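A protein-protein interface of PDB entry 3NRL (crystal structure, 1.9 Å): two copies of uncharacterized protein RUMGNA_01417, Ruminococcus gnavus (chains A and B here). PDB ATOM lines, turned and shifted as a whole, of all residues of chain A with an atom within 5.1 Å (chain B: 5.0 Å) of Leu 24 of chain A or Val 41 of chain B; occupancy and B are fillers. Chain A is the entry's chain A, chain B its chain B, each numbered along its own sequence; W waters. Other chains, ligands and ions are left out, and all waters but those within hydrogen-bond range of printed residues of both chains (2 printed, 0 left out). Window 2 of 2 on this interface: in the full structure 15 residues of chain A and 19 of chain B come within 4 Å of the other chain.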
ATOM      1  N   ARG A  21      -2.353 -22.958  12.047  1.00  0.00           N
ATOM      2  CA  ARG A  21      -3.196 -23.620  13.026  1.00  0.00           C
ATOM      3  C   ARG A  21      -2.289 -24.462  13.917  1.00  0.00           C
ATOM      4  O   ARG A  21      -1.643 -25.401  13.444  1.00  0.00           O
ATOM      5  CB  ARG A  21      -4.215 -24.528  12.347  1.00  0.00           C
ATOM      6  CG  ARG A  21      -4.976 -25.379  13.350  1.00  0.00           C
ATOM      7  CD  ARG A  21      -5.416 -26.692  12.741  1.00  0.00           C
ATOM      8  NE  ARG A  21      -6.634 -26.557  11.955  1.00  0.00           N
ATOM      9  CZ  ARG A  21      -7.798 -26.162  12.460  1.00  0.00           C
ATOM     10  NH1 ARG A  21      -7.880 -25.862  13.749  1.00  0.00           N
ATOM     11  NH2 ARG A  21      -8.875 -26.088  11.684  1.00  0.00           N
ATOM     12  N   PHE A  22      -2.243 -24.124  15.203  1.00  0.00           N
ATOM     13  CA  PHE A  22      -1.407 -24.850  16.150  1.00  0.00           C
ATOM     14  C   PHE A  22      -2.180 -25.955  16.858  1.00  0.00           C
ATOM     15  O   PHE A  22      -1.641 -27.024  17.138  1.00  0.00           O
ATOM     16  CB  PHE A  22      -0.846 -23.896  17.205  1.00  0.00           C
ATOM     17  CG  PHE A  22       0.121 -22.889  16.661  1.00  0.00           C
ATOM     18  CD1 PHE A  22       1.325 -23.292  16.097  1.00  0.00           C
ATOM     19  CD2 PHE A  22      -0.162 -21.531  16.733  1.00  0.00           C
ATOM     20  CE1 PHE A  22       2.235 -22.356  15.610  1.00  0.00           C
ATOM     21  CE2 PHE A  22       0.740 -20.586  16.250  1.00  0.00           C
ATOM     22  CZ  PHE A  22       1.940 -21.000  15.687  1.00  0.00           C
ATOM     23  N   ASP A  23      -3.445 -25.686  17.147  1.00  0.00           N
ATOM     24  CA  ASP A  23      -4.282 -26.647  17.846  1.00  0.00           C
ATOM     25  C   ASP A  23      -5.662 -26.659  17.208  1.00  0.00           C
ATOM     26  O   ASP A  23      -5.944 -25.864  16.312  1.00  0.00           O
ATOM     27  CB  ASP A  23      -4.394 -26.250  19.322  1.00  0.00           C
ATOM     28  CG  ASP A  23      -4.336 -27.438  20.252  1.00  0.00           C
ATOM     29  OD1 ASP A  23      -5.139 -28.378  20.071  1.00  0.00           O
ATOM     30  OD2 ASP A  23      -3.487 -27.430  21.169  1.00  0.00           O
ATOM     31  N   LEU A  24      -6.521 -27.555  17.675  1.00  0.00           N
ATOM     32  CA  LEU A  24      -7.872 -27.659  17.144  1.00  0.00           C
ATOM     33  C   LEU A  24      -8.545 -26.285  17.105  1.00  0.00           C
ATOM     34  O   LEU A  24      -9.270 -25.966  16.162  1.00  0.00           O
ATOM     35  CB  LEU A  24      -8.691 -28.631  18.001  1.00  0.00           C
ATOM     36  CG  LEU A  24     -10.048 -29.075  17.458  1.00  0.00           C
ATOM     37  CD1 LEU A  24      -9.882 -29.659  16.065  1.00  0.00           C
ATOM     38  CD2 LEU A  24     -10.659 -30.105  18.399  1.00  0.00           C
ATOM     39  N   GLU A  25      -8.293 -25.468  18.123  1.00  0.00           N
ATOM     40  CA  GLU A  25      -8.877 -24.131  18.189  1.00  0.00           C
ATOM     41  C   GLU A  25      -7.867 -23.068  18.612  1.00  0.00           C
ATOM     42  O   GLU A  25      -8.184 -22.165  19.386  1.00  0.00           O
ATOM     43  CB  GLU A  25     -10.068 -24.118  19.150  1.00  0.00           C
ATOM     44  CG  GLU A  25     -11.337 -24.720  18.571  1.00  0.00           C
ATOM     45  CD  GLU A  25     -11.784 -24.018  17.299  1.00  0.00           C
ATOM     46  OE1 GLU A  25     -11.920 -22.775  17.318  1.00  0.00           O
ATOM     47  OE2 GLU A  25     -12.004 -24.709  16.281  1.00  0.00           O
ATOM     48  N   SER A  26      -6.649 -23.181  18.096  1.00  0.00           N
ATOM     49  CA  SER A  26      -5.586 -22.232  18.405  1.00  0.00           C
ATOM     50  C   SER A  26      -4.907 -21.841  17.099  1.00  0.00           C
ATOM     51  O   SER A  26      -4.281 -22.678  16.449  1.00  0.00           O
ATOM     52  CB  SER A  26      -4.574 -22.875  19.353  1.00  0.00           C
ATOM     53  OG  SER A  26      -3.486 -22.002  19.599  1.00  0.00           O
ATOM     54  N   PHE A  27      -5.039 -20.569  16.724  1.00  0.00           N
ATOM     55  CA  PHE A  27      -4.466 -20.057  15.482  1.00  0.00           C
ATOM     56  C   PHE A  27      -3.488 -18.917  15.751  1.00  0.00           C
ATOM     57  O   PHE A  27      -3.585 -18.238  16.774  1.00  0.00           O
ATOM     58  CB  PHE A  27      -5.591 -19.559  14.570  1.00  0.00           C
ATOM     59  CG  PHE A  27      -6.574 -20.629  14.180  1.00  0.00           C
ATOM     60  CD1 PHE A  27      -6.474 -21.266  12.948  1.00  0.00           C
ATOM     61  CD2 PHE A  27      -7.592 -21.009  15.049  1.00  0.00           C
ATOM     62  CE1 PHE A  27      -7.371 -22.266  12.584  1.00  0.00           C
ATOM     63  CE2 PHE A  27      -8.496 -22.012  14.695  1.00  0.00           C
ATOM     64  CZ  PHE A  27      -8.386 -22.642  13.458  1.00  0.00           C
ATOM     65  N   VAL B  39      -8.833 -37.446  12.158  1.00  0.00           N
ATOM     66  CA  VAL B  39      -8.366 -36.098  12.446  1.00  0.00           C
ATOM     67  C   VAL B  39      -7.679 -36.162  13.812  1.00  0.00           C
ATOM     68  O   VAL B  39      -8.188 -36.791  14.745  1.00  0.00           O
ATOM     69  CB  VAL B  39      -9.535 -35.091  12.514  1.00  0.00           C
ATOM     70  CG1 VAL B  39      -9.034 -33.735  13.008  1.00  0.00           C
ATOM     71  CG2 VAL B  39     -10.181 -34.944  11.130  1.00  0.00           C
ATOM     72  N   LYS B  40      -6.516 -35.534  13.925  1.00  0.00           N
ATOM     73  CA  LYS B  40      -5.792 -35.538  15.190  1.00  0.00           C
ATOM     74  C   LYS B  40      -6.336 -34.481  16.134  1.00  0.00           C
ATOM     75  O   LYS B  40      -6.327 -33.296  15.821  1.00  0.00           O
ATOM     76  CB  LYS B  40      -4.297 -35.284  14.967  1.00  0.00           C
ATOM     77  CG  LYS B  40      -3.554 -36.448  14.346  1.00  0.00           C
ATOM     78  CD  LYS B  40      -3.865 -36.587  12.865  1.00  0.00           C
ATOM     79  CE  LYS B  40      -3.855 -38.040  12.452  1.00  0.00           C
ATOM     80  NZ  LYS B  40      -4.986 -38.758  13.105  1.00  0.00           N
ATOM     81  N   VAL B  41      -6.828 -34.924  17.286  1.00  0.00           N
ATOM     82  CA  VAL B  41      -7.350 -34.027  18.310  1.00  0.00           C
ATOM     83  C   VAL B  41      -6.566 -34.419  19.555  1.00  0.00           C
ATOM     84  O   VAL B  41      -6.734 -35.526  20.071  1.00  0.00           O
ATOM     85  CB  VAL B  41      -8.857 -34.249  18.557  1.00  0.00           C
ATOM     86  CG1 VAL B  41      -9.354 -33.301  19.638  1.00  0.00           C
ATOM     87  CG2 VAL B  41      -9.637 -34.023  17.270  1.00  0.00           C
ATOM     88  N   LYS B  42      -5.703 -33.521  20.025  1.00  0.00           N
ATOM     89  CA  LYS B  42      -4.863 -33.809  21.184  1.00  0.00           C
ATOM     90  C   LYS B  42      -3.895 -34.907  20.759  1.00  0.00           C
ATOM     91  O   LYS B  42      -3.102 -34.721  19.838  1.00  0.00           O
ATOM     92  CB  LYS B  42      -5.713 -34.287  22.366  1.00  0.00           C
ATOM     93  CG  LYS B  42      -6.308 -33.175  23.218  1.00  0.00           C
ATOM     94  CD  LYS B  42      -5.245 -32.534  24.100  1.00  0.00           C
ATOM     95  CE  LYS B  42      -5.861 -31.580  25.111  1.00  0.00           C
ATOM     96  NZ  LYS B  42      -4.840 -31.005  26.032  1.00  0.00           N
ATOM     97  N   ASP B  43      -3.963 -36.053  21.425  1.00  0.00           N
ATOM     98  CA  ASP B  43      -3.098 -37.171  21.079  1.00  0.00           C
ATOM     99  C   ASP B  43      -3.958 -38.393  20.768  1.00  0.00           C
ATOM    100  O   ASP B  43      -3.643 -39.517  21.154  1.00  0.00           O
ATOM    101  CB  ASP B  43      -2.125 -37.469  22.224  1.00  0.00           C
ATOM    102  CG  ASP B  43      -1.107 -36.354  22.428  1.00  0.00           C
ATOM    103  OD1 ASP B  43      -0.371 -36.034  21.468  1.00  0.00           O
ATOM    104  OD2 ASP B  43      -1.044 -35.798  23.545  1.00  0.00           O
ATOM    105  N   VAL B  44      -5.053 -38.147  20.058  1.00  0.00           N
ATOM    106  CA  VAL B  44      -5.989 -39.190  19.669  1.00  0.00           C
ATOM    107  C   VAL B  44      -6.446 -38.945  18.235  1.00  0.00           C
ATOM    108  O   VAL B  44      -6.513 -37.799  17.787  1.00  0.00           O
ATOM    109  CB  VAL B  44      -7.223 -39.185  20.598  1.00  0.00           C
ATOM    110  CG1 VAL B  44      -8.280 -40.146  20.080  1.00  0.00           C
ATOM    111  CG2 VAL B  44      -6.804 -39.568  22.010  1.00  0.00           C
ATOM    112  N   VAL B  46      -9.441 -39.081  15.656  1.00  0.00           N
ATOM    113  CA  VAL B  46     -10.897 -39.134  15.598  1.00  0.00           C
ATOM    114  C   VAL B  46     -11.392 -39.460  14.192  1.00  0.00           C
ATOM    115  O   VAL B  46     -11.057 -38.771  13.225  1.00  0.00           O
ATOM    116  CB  VAL B  46     -11.518 -37.795  16.040  1.00  0.00           C
ATOM    117  CG1 VAL B  46     -13.038 -37.891  16.004  1.00  0.00           C
ATOM    118  CG2 VAL B  46     -11.033 -37.432  17.437  1.00  0.00           C
ATOM    119  N   LEU B  61     -16.790 -34.756  13.859  1.00  0.00           N
ATOM    120  CA  LEU B  61     -16.036 -33.726  14.562  1.00  0.00           C
ATOM    121  C   LEU B  61     -16.562 -32.323  14.284  1.00  0.00           C
ATOM    122  O   LEU B  61     -16.553 -31.860  13.141  1.00  0.00           O
ATOM    123  CB  LEU B  61     -14.553 -33.797  14.174  1.00  0.00           C
ATOM    124  CG  LEU B  61     -13.654 -32.756  14.846  1.00  0.00           C
ATOM    125  CD1 LEU B  61     -13.640 -32.989  16.355  1.00  0.00           C
ATOM    126  CD2 LEU B  61     -12.239 -32.848  14.271  1.00  0.00           C
ATOM    127  N   VAL B  63     -15.918 -28.741  14.311  1.00  0.00           N
ATOM    128  CA  VAL B  63     -14.830 -27.779  14.361  1.00  0.00           C
ATOM    129  C   VAL B  63     -15.223 -26.522  13.600  1.00  0.00           C
ATOM    130  O   VAL B  63     -15.973 -26.587  12.626  1.00  0.00           O
ATOM    131  CB  VAL B  63     -13.551 -28.365  13.737  1.00  0.00           C
ATOM    132  CG1 VAL B  63     -13.792 -28.681  12.267  1.00  0.00           C
ATOM    133  CG2 VAL B  63     -12.398 -27.388  13.897  1.00  0.00           C
ATOM    134  N   SER B  64     -14.711 -25.381  14.052  1.00  0.00           N
ATOM    135  CA  SER B  64     -15.001 -24.097  13.425  1.00  0.00           C
ATOM    136  C   SER B  64     -14.644 -24.094  11.940  1.00  0.00           C
ATOM    137  O   SER B  64     -15.395 -23.577  11.114  1.00  0.00           O
ATOM    138  CB  SER B  64     -14.232 -22.978  14.142  1.00  0.00           C
ATOM    139  OG  SER B  64     -12.833 -23.208  14.099  1.00  0.00           O
ATOM    140  N   LEU B  69      -6.126 -28.917   9.661  1.00  0.00           N
ATOM    141  CA  LEU B  69      -6.234 -30.069  10.547  1.00  0.00           C
ATOM    142  C   LEU B  69      -5.205 -31.123  10.157  1.00  0.00           C
ATOM    143  O   LEU B  69      -4.880 -31.277   8.976  1.00  0.00           O
ATOM    144  CB  LEU B  69      -7.631 -30.683  10.456  1.00  0.00           C
ATOM    145  CG  LEU B  69      -8.800 -29.869  11.020  1.00  0.00           C
ATOM    146  CD1 LEU B  69     -10.105 -30.623  10.756  1.00  0.00           C
ATOM    147  CD2 LEU B  69      -8.607 -29.641  12.517  1.00  0.00           C
HETATM  148  O   HOH W   1      -5.601 -30.659  18.902  1.00  0.00           O
HETATM  149  O   HOH W   2     -14.921 -24.609  17.042  1.00  0.00           O
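Water W1 lies within hydrogen-bond range of OD1 of Asp 23 of chain A (2.6 Å), N of Lys 42 of chain B (3.1 Å) and N of Leu 24 of chain A (3.5 Å). Water W2 bridges OE2 of Glu 25 of chain A and N of Ser 64 of chain B.
CD2 of Leu 24 of chain A touches CG1 of Val 41 of chain B, 3.7 Å away. CD1 of Leu 24 of chain A touches CD2 of Leu 69 of chain B, 3.8 Å away. Val 63 of chain B touches Glu 25 of chain A (CG2 to OE2, 3.6 Å).
Of chain B, only Val 41 and Leu 69 come within 4 Å of Leu 24 of chain A. Val 41 of chain B touches one residue of chain A. Of the printed residues of chain B, Glu 25 of chain A touches Val 63 and Ser 64. Printed residues of chain A within 4 Å of Val 63 of chain B: Glu 25. Lys 40 of chain B touches none of the printed residues of chain A. Leu 61 of chain B touches none of the printed residues of chain A. The nearest printed residue of chain A that does not touch Val 41 of chain B is Asp 23 of chain A (6.2 Å).
No position is printed for both chains. Of the 5 pairs that touch across the chains among the printed residues, none has its exchanged pair printed and touching as well.
NH1 of Arg 21 of chain A sits close to O of Asp 23 of chain A. The guanidinium group (NH1) of Arg 21 of chain A sits at hydrogen-bond distance from the backbone carbonyl oxygen (O) of Leu 24 of chain A, at 2.8 Å.
The side-chain carboxylate of Glu 25 of chain A is in hydrogen-bond range of the side-chain hydroxyl of Ser 64 of chain B (2.8 Å). NE of Arg 21 of chain A lies close to N of Leu 69 of chain B, 3.3 Å away.
Hydrophobic or aromatic side chains of chain B within 4 Å of the printed part of chain A: Val 41, Val 63 and Leu 69. Among the printed residues, no Asp or Glu carboxylate lies within 4 Å of a Lys or Arg side-chain nitrogen of the other chain.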
